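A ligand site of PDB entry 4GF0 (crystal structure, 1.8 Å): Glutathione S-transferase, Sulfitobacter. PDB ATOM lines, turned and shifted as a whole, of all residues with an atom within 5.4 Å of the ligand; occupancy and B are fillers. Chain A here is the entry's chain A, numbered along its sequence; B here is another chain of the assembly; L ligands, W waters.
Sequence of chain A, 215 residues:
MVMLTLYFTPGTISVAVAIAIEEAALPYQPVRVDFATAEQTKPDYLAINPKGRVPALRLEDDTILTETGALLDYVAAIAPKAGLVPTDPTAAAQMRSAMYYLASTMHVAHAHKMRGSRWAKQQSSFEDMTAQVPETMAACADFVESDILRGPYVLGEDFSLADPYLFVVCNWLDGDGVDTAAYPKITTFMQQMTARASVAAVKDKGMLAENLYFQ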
ATOM      1  N   THR A  12       1.904  36.517 -18.545  1.00  0.00           N
ATOM      2  CA  THR A  12       2.141  35.080 -18.675  1.00  0.00           C
ATOM      3  C   THR A  12       3.626  34.759 -18.717  1.00  0.00           C
ATOM      4  O   THR A  12       4.484  35.656 -18.778  1.00  0.00           O
ATOM      5  CB  THR A  12       1.446  34.469 -19.913  1.00  0.00           C
ATOM      6  OG1 THR A  12       2.059  34.977 -21.111  1.00  0.00           O
ATOM      7  CG2 THR A  12      -0.050  34.808 -19.917  1.00  0.00           C
ATOM      8  N   ILE A  13       3.931  33.456 -18.744  1.00  0.00           N
ATOM      9  CA  ILE A  13       5.311  32.995 -18.729  1.00  0.00           C
ATOM     10  C   ILE A  13       6.085  33.404 -19.981  1.00  0.00           C
ATOM     11  O   ILE A  13       7.321  33.461 -19.959  1.00  0.00           O
ATOM     12  CB  ILE A  13       5.374  31.457 -18.526  1.00  0.00           C
ATOM     13  CG1 ILE A  13       6.767  31.037 -18.016  1.00  0.00           C
ATOM     14  CG2 ILE A  13       4.971  30.711 -19.805  1.00  0.00           C
ATOM     15  CD1 ILE A  13       7.139  31.722 -16.696  1.00  0.00           C
ATOM     16  N   SER A  14       5.373  33.699 -21.063  1.00  0.00           N
ATOM     17  CA  SER A  14       6.011  34.182 -22.296  1.00  0.00           C
ATOM     18  C   SER A  14       6.848  35.425 -22.060  1.00  0.00           C
ATOM     19  O   SER A  14       7.791  35.698 -22.803  1.00  0.00           O
ATOM     20  CB  SER A  14       4.958  34.490 -23.368  1.00  0.00           C
ATOM     21  OG  SER A  14       3.968  35.396 -22.881  1.00  0.00           O
ATOM     22  N   PHE A  35      -6.028  36.305 -24.669  1.00  0.00           N
ATOM     23  CA  PHE A  35      -6.731  35.256 -23.923  1.00  0.00           C
ATOM     24  C   PHE A  35      -8.200  35.604 -23.680  1.00  0.00           C
ATOM     25  O   PHE A  35      -9.015  34.718 -23.432  1.00  0.00           O
ATOM     26  CB  PHE A  35      -6.075  35.026 -22.550  1.00  0.00           C
ATOM     27  CG  PHE A  35      -4.808  34.226 -22.595  1.00  0.00           C
ATOM     28  CD1 PHE A  35      -4.141  33.984 -23.786  1.00  0.00           C
ATOM     29  CD2 PHE A  35      -4.272  33.720 -21.418  1.00  0.00           C
ATOM     30  CE1 PHE A  35      -2.961  33.246 -23.816  1.00  0.00           C
ATOM     31  CE2 PHE A  35      -3.091  32.983 -21.431  1.00  0.00           C
ATOM     32  CZ  PHE A  35      -2.439  32.740 -22.638  1.00  0.00           C
ATOM     33  N   GLN A  40      -5.731  31.949 -28.362  1.00  0.00           N
ATOM     34  CA  GLN A  40      -4.733  30.872 -28.336  1.00  0.00           C
ATOM     35  C   GLN A  40      -5.349  29.500 -28.618  1.00  0.00           C
ATOM     36  O   GLN A  40      -4.623  28.537 -28.895  1.00  0.00           O
ATOM     37  CB  GLN A  40      -3.988  30.864 -26.999  1.00  0.00           C
ATOM     38  CG  GLN A  40      -4.739  30.227 -25.818  1.00  0.00           C
ATOM     39  CD  GLN A  40      -5.759  31.157 -25.162  1.00  0.00           C
ATOM     40  OE1 GLN A  40      -6.104  32.209 -25.711  1.00  0.00           O
ATOM     41  NE2 GLN A  40      -6.242  30.764 -23.981  1.00  0.00           N
ATOM     42  N   THR A  41      -6.669  29.399 -28.567  1.00  0.00           N
ATOM     43  CA  THR A  41      -7.373  28.123 -28.754  1.00  0.00           C
ATOM     44  C   THR A  41      -7.941  27.958 -30.161  1.00  0.00           C
ATOM     45  O   THR A  41      -8.515  26.921 -30.487  1.00  0.00           O
ATOM     46  CB  THR A  41      -8.555  27.983 -27.767  1.00  0.00           C
ATOM     47  OG1 THR A  41      -9.606  28.860 -28.167  1.00  0.00           O
ATOM     48  CG2 THR A  41      -8.120  28.324 -26.353  1.00  0.00           C
ATOM     49  N   GLY A  52      -1.412  25.393 -28.305  1.00  0.00           N
ATOM     50  CA  GLY A  52      -2.311  26.465 -27.933  1.00  0.00           C
ATOM     51  C   GLY A  52      -1.823  27.239 -26.721  1.00  0.00           C
ATOM     52  O   GLY A  52      -2.643  27.686 -25.904  1.00  0.00           O
ATOM     53  N   ARG A  53      -0.511  27.394 -26.594  1.00  0.00           N
ATOM     54  CA  ARG A  53       0.073  28.103 -25.450  1.00  0.00           C
ATOM     55  C   ARG A  53       0.995  29.199 -25.938  1.00  0.00           C
ATOM     56  O   ARG A  53       1.483  29.145 -27.067  1.00  0.00           O
ATOM     57  CB  ARG A  53       0.897  27.160 -24.564  1.00  0.00           C
ATOM     58  CG  ARG A  53       0.234  25.852 -24.213  1.00  0.00           C
ATOM     59  CD  ARG A  53      -0.940  26.010 -23.248  1.00  0.00           C
ATOM     60  NE  ARG A  53      -1.462  24.681 -22.908  1.00  0.00           N
ATOM     61  CZ  ARG A  53      -0.884  23.867 -22.032  1.00  0.00           C
ATOM     62  NH1 ARG A  53       0.208  24.260 -21.395  1.00  0.00           N
ATOM     63  NH2 ARG A  53      -1.405  22.665 -21.797  1.00  0.00           N
ATOM     64  N   VAL A  54       1.249  30.168 -25.065  1.00  0.00           N
ATOM     65  CA  VAL A  54       2.349  31.099 -25.281  1.00  0.00           C
ATOM     66  C   VAL A  54       3.416  30.767 -24.227  1.00  0.00           C
ATOM     67  O   VAL A  54       3.077  30.306 -23.130  1.00  0.00           O
ATOM     68  CB  VAL A  54       1.895  32.592 -25.177  1.00  0.00           C
ATOM     69  CG1 VAL A  54       0.923  32.925 -26.292  1.00  0.00           C
ATOM     70  CG2 VAL A  54       1.249  32.848 -23.820  1.00  0.00           C
ATOM     71  N   PRO A  55       4.703  30.982 -24.531  1.00  0.00           N
ATOM     72  CA  PRO A  55       5.276  31.616 -25.720  1.00  0.00           C
ATOM     73  C   PRO A  55       5.425  30.698 -26.931  1.00  0.00           C
ATOM     74  O   PRO A  55       5.471  29.476 -26.795  1.00  0.00           O
ATOM     75  CB  PRO A  55       6.673  32.016 -25.253  1.00  0.00           C
ATOM     76  CG  PRO A  55       7.022  30.917 -24.256  1.00  0.00           C
ATOM     77  CD  PRO A  55       5.736  30.679 -23.521  1.00  0.00           C
ATOM     78  N   GLU A  67       8.028  26.222 -25.843  1.00  0.00           N
ATOM     79  CA  GLU A  67       8.490  25.870 -24.476  1.00  0.00           C
ATOM     80  C   GLU A  67       9.467  26.900 -23.927  1.00  0.00           C
ATOM     81  O   GLU A  67      10.594  27.022 -24.399  1.00  0.00           O
ATOM     82  CB  GLU A  67       9.066  24.462 -24.363  1.00  0.00           C
ATOM     83  CG  GLU A  67       8.084  23.345 -24.756  1.00  0.00           C
ATOM     84  CD  GLU A  67       6.916  23.197 -23.775  1.00  0.00           C
ATOM     85  OE1 GLU A  67       7.052  23.593 -22.589  1.00  0.00           O
ATOM     86  OE2 GLU A  67       5.869  22.666 -24.194  1.00  0.00           O
ATOM     87  N   THR A  68       9.017  27.620 -22.919  1.00  0.00           N
ATOM     88  CA  THR A  68       9.786  28.729 -22.356  1.00  0.00           C
ATOM     89  C   THR A  68      11.266  28.371 -22.136  1.00  0.00           C
ATOM     90  O   THR A  68      12.147  29.116 -22.573  1.00  0.00           O
ATOM     91  CB  THR A  68       9.151  29.175 -21.039  1.00  0.00           C
ATOM     92  OG1 THR A  68       7.807  29.617 -21.305  1.00  0.00           O
ATOM     93  CG2 THR A  68       9.932  30.332 -20.405  1.00  0.00           C
ATOM     94  N   GLY A  69      11.544  27.253 -21.479  1.00  0.00           N
ATOM     95  CA  GLY A  69      12.925  26.934 -21.147  1.00  0.00           C
ATOM     96  C   GLY A  69      13.786  26.730 -22.386  1.00  0.00           C
ATOM     97  O   GLY A  69      14.964  27.093 -22.416  1.00  0.00           O
ATOM     98  N   ALA A 103       9.314  24.842 -14.675  1.00  0.00           N
ATOM     99  CA  ALA A 103       8.512  24.246 -15.748  1.00  0.00           C
ATOM    100  C   ALA A 103       7.639  23.081 -15.301  1.00  0.00           C
ATOM    101  O   ALA A 103       6.517  22.920 -15.780  1.00  0.00           O
ATOM    102  CB  ALA A 103       9.416  23.802 -16.908  1.00  0.00           C
ATOM    103  N   HIS A 107       5.188  26.321 -12.078  1.00  0.00           N
ATOM    104  CA  HIS A 107       4.215  26.787 -13.066  1.00  0.00           C
ATOM    105  C   HIS A 107       3.035  25.830 -13.051  1.00  0.00           C
ATOM    106  O   HIS A 107       1.884  26.243 -13.145  1.00  0.00           O
ATOM    107  CB  HIS A 107       4.825  26.868 -14.467  1.00  0.00           C
ATOM    108  CG  HIS A 107       3.955  27.582 -15.476  1.00  0.00           C
ATOM    109  ND1 HIS A 107       4.412  27.934 -16.722  1.00  0.00           N
ATOM    110  CD2 HIS A 107       2.661  27.990 -15.408  1.00  0.00           C
ATOM    111  CE1 HIS A 107       3.447  28.539 -17.388  1.00  0.00           C
ATOM    112  NE2 HIS A 107       2.375  28.585 -16.622  1.00  0.00           N
ATOM    113  N   ARG A 115      -6.628  26.397 -15.074  1.00  0.00           N
ATOM    114  CA  ARG A 115      -6.613  25.396 -16.131  1.00  0.00           C
ATOM    115  C   ARG A 115      -6.817  23.992 -15.587  1.00  0.00           C
ATOM    116  O   ARG A 115      -6.261  23.029 -16.122  1.00  0.00           O
ATOM    117  CB  ARG A 115      -5.306  25.455 -16.939  1.00  0.00           C
ATOM    118  CG  ARG A 115      -4.868  26.848 -17.321  1.00  0.00           C
ATOM    119  CD  ARG A 115      -5.851  27.508 -18.261  1.00  0.00           C
ATOM    120  NE  ARG A 115      -5.409  28.853 -18.624  1.00  0.00           N
ATOM    121  CZ  ARG A 115      -6.136  29.732 -19.300  1.00  0.00           C
ATOM    122  NH1 ARG A 115      -7.365  29.420 -19.686  1.00  0.00           N
ATOM    123  NH2 ARG A 115      -5.647  30.931 -19.584  1.00  0.00           N
ATOM    124  N   ARG A 118      -7.503  20.839 -17.748  1.00  0.00           N
ATOM    125  CA  ARG A 118      -6.449  20.031 -18.373  1.00  0.00           C
ATOM    126  C   ARG A 118      -6.418  18.599 -17.830  1.00  0.00           C
ATOM    127  O   ARG A 118      -5.998  17.684 -18.530  1.00  0.00           O
ATOM    128  CB  ARG A 118      -5.083  20.670 -18.172  1.00  0.00           C
ATOM    129  CG  ARG A 118      -4.896  21.955 -18.958  1.00  0.00           C
ATOM    130  CD  ARG A 118      -3.503  22.486 -18.736  1.00  0.00           C
ATOM    131  NE  ARG A 118      -3.328  23.814 -19.308  1.00  0.00           N
ATOM    132  CZ  ARG A 118      -2.302  24.616 -19.035  1.00  0.00           C
ATOM    133  NH1 ARG A 118      -1.351  24.211 -18.199  1.00  0.00           N
ATOM    134  NH2 ARG A 118      -2.228  25.822 -19.598  1.00  0.00           N
ATOM    135  N   TYR A 165      12.922  33.688 -15.865  1.00  0.00           N
ATOM    136  CA  TYR A 165      11.971  32.608 -15.625  1.00  0.00           C
ATOM    137  C   TYR A 165      11.414  32.710 -14.197  1.00  0.00           C
ATOM    138  O   TYR A 165      10.194  32.713 -14.015  1.00  0.00           O
ATOM    139  CB  TYR A 165      12.666  31.257 -15.849  1.00  0.00           C
ATOM    140  CG  TYR A 165      11.756  30.135 -16.312  1.00  0.00           C
ATOM    141  CD1 TYR A 165      10.397  30.127 -16.013  1.00  0.00           C
ATOM    142  CD2 TYR A 165      12.278  29.068 -17.035  1.00  0.00           C
ATOM    143  CE1 TYR A 165       9.573  29.076 -16.440  1.00  0.00           C
ATOM    144  CE2 TYR A 165      11.467  28.034 -17.470  1.00  0.00           C
ATOM    145  CZ  TYR A 165      10.123  28.034 -17.167  1.00  0.00           C
ATOM    146  OH  TYR A 165       9.355  26.976 -17.604  1.00  0.00           O
ATOM    147  N   TRP A 172       3.486  35.913  -9.943  1.00  0.00           N
ATOM    148  CA  TRP A 172       2.159  35.323  -9.755  1.00  0.00           C
ATOM    149  C   TRP A 172       1.808  35.121  -8.282  1.00  0.00           C
ATOM    150  O   TRP A 172       0.650  34.880  -7.959  1.00  0.00           O
ATOM    151  CB  TRP A 172       2.069  33.957 -10.435  1.00  0.00           C
ATOM    152  CG  TRP A 172       2.106  33.962 -11.924  1.00  0.00           C
ATOM    153  CD1 TRP A 172       1.654  34.955 -12.751  1.00  0.00           C
ATOM    154  CD2 TRP A 172       2.610  32.925 -12.769  1.00  0.00           C
ATOM    155  NE1 TRP A 172       1.854  34.595 -14.060  1.00  0.00           N
ATOM    156  CE2 TRP A 172       2.432  33.355 -14.100  1.00  0.00           C
ATOM    157  CE3 TRP A 172       3.184  31.683 -12.525  1.00  0.00           C
ATOM    158  CZ2 TRP A 172       2.835  32.572 -15.195  1.00  0.00           C
ATOM    159  CZ3 TRP A 172       3.574  30.900 -13.601  1.00  0.00           C
ATOM    160  CH2 TRP A 172       3.397  31.347 -14.921  1.00  0.00           C
ATOM    161  N   TYR B 100      11.334  19.943 -22.392  1.00  0.00           N
ATOM    162  CA  TYR B 100      10.449  20.733 -21.537  1.00  0.00           C
ATOM    163  C   TYR B 100       8.988  20.325 -21.690  1.00  0.00           C
ATOM    164  O   TYR B 100       8.205  20.428 -20.742  1.00  0.00           O
ATOM    165  CB  TYR B 100      10.611  22.236 -21.786  1.00  0.00           C
ATOM    166  CG  TYR B 100      11.794  22.836 -21.069  1.00  0.00           C
ATOM    167  CD1 TYR B 100      11.687  23.254 -19.742  1.00  0.00           C
ATOM    168  CD2 TYR B 100      13.028  22.975 -21.701  1.00  0.00           C
ATOM    169  CE1 TYR B 100      12.776  23.812 -19.067  1.00  0.00           C
ATOM    170  CE2 TYR B 100      14.117  23.533 -21.026  1.00  0.00           C
ATOM    171  CZ  TYR B 100      13.980  23.949 -19.714  1.00  0.00           C
ATOM    172  OH  TYR B 100      15.060  24.510 -19.062  1.00  0.00           O
ATOM    173  N   SER B 104       6.870  19.325 -18.433  1.00  0.00           N
ATOM    174  CA  SER B 104       5.801  20.233 -18.020  1.00  0.00           C
ATOM    175  C   SER B 104       4.414  19.722 -18.348  1.00  0.00           C
ATOM    176  O   SER B 104       3.418  20.175 -17.761  1.00  0.00           O
ATOM    177  CB  SER B 104       5.982  21.606 -18.682  1.00  0.00           C
ATOM    178  OG  SER B 104       5.859  21.495 -20.093  1.00  0.00           O
ATOM    179  N   THR B 105       4.329  18.808 -19.296  1.00  0.00           N
ATOM    180  CA  THR B 105       3.028  18.401 -19.811  1.00  0.00           C
ATOM    181  C   THR B 105       2.803  16.917 -19.720  1.00  0.00           C
ATOM    182  O   THR B 105       1.859  16.459 -19.060  1.00  0.00           O
ATOM    183  CB  THR B 105       2.839  18.874 -21.265  1.00  0.00           C
ATOM    184  OG1 THR B 105       2.984  20.292 -21.323  1.00  0.00           O
ATOM    185  CG2 THR B 105       1.460  18.485 -21.768  1.00  0.00           C
HETATM  186  N1  LIG L   1       5.225  24.360 -20.639  1.00  0.00           N
HETATM  187  C1  LIG L   1       4.849  25.584 -21.310  1.00  0.00           C
HETATM  188  C2  LIG L   1       6.001  26.532 -21.328  1.00  0.00           C
HETATM  189  O1  LIG L   1       6.182  27.295 -22.318  1.00  0.00           O
HETATM  190  O2  LIG L   1       6.778  26.602 -20.341  1.00  0.00           O
HETATM  191  C3  LIG L   1       3.709  26.256 -20.578  1.00  0.00           C
HETATM  192  C4  LIG L   1       3.046  27.233 -21.561  1.00  0.00           C
HETATM  193  C5  LIG L   1       1.731  27.727 -20.956  1.00  0.00           C
HETATM  194  O3  LIG L   1       0.946  26.952 -20.397  1.00  0.00           O
HETATM  195  N2  LIG L   1       1.411  29.146 -21.056  1.00  0.00           N
HETATM  196  C6  LIG L   1       0.170  29.637 -20.504  1.00  0.00           C
HETATM  197  C7  LIG L   1      -0.878  29.555 -21.596  1.00  0.00           C
HETATM  198  O4  LIG L   1      -0.556  29.673 -22.766  1.00  0.00           O
HETATM  199  C8  LIG L   1       0.303  31.047 -20.044  1.00  0.00           C
HETATM  200  S1  LIG L   1       1.399  31.135 -18.643  1.00  0.00           S
HETATM  201  N3  LIG L   1      -2.277  29.320 -21.276  1.00  0.00           N
HETATM  202  C9  LIG L   1      -3.242  29.274 -22.371  1.00  0.00           C
HETATM  203  C10 LIG L   1      -4.272  28.203 -22.142  1.00  0.00           C
HETATM  204  O5  LIG L   1      -4.070  27.278 -21.303  1.00  0.00           O
HETATM  205  O6  LIG L   1      -5.358  28.205 -22.806  1.00  0.00           O
HETATM  206  O   HOH W   1      -4.966  26.555 -25.130  1.00  0.00           O
HETATM  207  O   HOH W   2       6.803  27.070 -17.769  1.00  0.00           O
HETATM  208  O   HOH W   3       5.221  24.644 -17.474  1.00  0.00           O
HETATM  209  O   HOH W   4       3.407  23.769 -23.804  1.00  0.00           O
HETATM  210  O   HOH W   5      -5.269  24.875 -21.169  1.00  0.00           O
HETATM  211  O   HOH W   6       5.532  27.345 -25.016  1.00  0.00           O
HETATM  212  O   HOH W   7       0.598  26.227 -17.760  1.00  0.00           O
HETATM  213  O   HOH W   8      -7.896  27.274 -22.714  1.00  0.00           O
HETATM  214  O   HOH W   9       9.576  25.619 -20.237  1.00  0.00           O
HETATM  215  O   HOH W  10       2.654  22.965 -20.038  1.00  0.00           O
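OE1 of Glu 67 is in salt-bridge range of N1 of the ligand.
N of Val 54 sits at hydrogen-bond distance from O4 of the ligand.
The backbone carbonyl oxygen (O) of Val 54 sits at hydrogen-bond distance from a nitrogen (N2) of the ligand, 2.9 Å away.
The guanidinium group (NH2) of Arg 118 lies within salt-bridge range of an oxygen (O5) of the ligand, 2.9 Å away.
The backbone NH (N) of Thr 68 sits at hydrogen-bond distance from an oxygen (O1) of the ligand (2.9 Å).
The side-chain hydroxyl of Thr 68 lies within hydrogen-bond range of an oxygen (O1) of the ligand (3.0 Å).
NE2 of Gln 40 sits at hydrogen-bond distance from O6 of the ligand (3.0 Å).
O3 of the ligand lies within hydrogen-bond range of NH1 of Arg 53, at 3.0 Å.
OG of Ser 104 of chain B is in hydrogen-bond range of N1 of the ligand, 3.0 Å away.
The guanidinium group (NE) of Arg 115 is in salt-bridge range of an oxygen (O5) of the ligand (3.4 Å).
S1 of the ligand lies close to NE2 of His 107.
S1 of the ligand sits close to N of Ile 13.
OE1 of Glu 67 lies within hydrogen-bond range of OG of Ser 104 of chain B, at 3.5 Å.
OG of Ser 104 of chain B lies close to OG1 of Thr 105 of chain B.
The side-chain hydroxyl of Ser 104 of chain B sits at hydrogen-bond distance from the backbone carbonyl oxygen of Tyr 100 of chain B (2.7 Å).
The side-chain hydroxyl of Ser 14 is in hydrogen-bond range of the side-chain hydroxyl of Thr 12.
Merely in contact with the ligand: Thr 12, Phe 35, Gly 52, Pro 55 and Tyr 165.
15 residues have an atom within 4 Å of the ligand: Thr 12, Ile 13, Phe 35, Gln 40, Gly 52, Arg 53, Val 54, Pro 55, Glu 67, Thr 68, His 107, Arg 115, Arg 118, Tyr 165 and Ser 104 of chain B.
The nearest printed residue that does not touch the ligand is Trp 172 (4.002 Å).
Water W2 lies within hydrogen-bond range of OH of Tyr 165 (2.6 Å), O2 of the ligand (2.6 Å) and ND1 of His 107 (2.7 Å).
Water W7 lies within hydrogen-bond range of an oxygen (O3) of the ligand, the guanidinium group of Arg 118 and a ring nitrogen (NE2) of His 107.
Water W6 lies within hydrogen-bond range of O of Pro 55, O1 of the ligand and N of Glu 67.
Water W9 lies within hydrogen-bond range of the backbone NH of Gly 69 (2.8 Å), an oxygen (O2) of the ligand (3.0 Å), the side-chain hydroxyl of Tyr 165 (3.0 Å) and the backbone NH of Thr 68 (3.4 Å).
Water W10 lies within hydrogen-bond range of the side-chain hydroxyl (OG1) of Thr 105 of chain B (3.0 Å), a nitrogen (N1) of the ligand (3.0 Å) and the guanidinium group (NH1) of Arg 53 (3.1 Å).
Water W3 lies within hydrogen-bond range of O of Ala 103 (2.7 Å), N1 of the ligand (3.2 Å) and ND1 of His 107 (3.5 Å).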
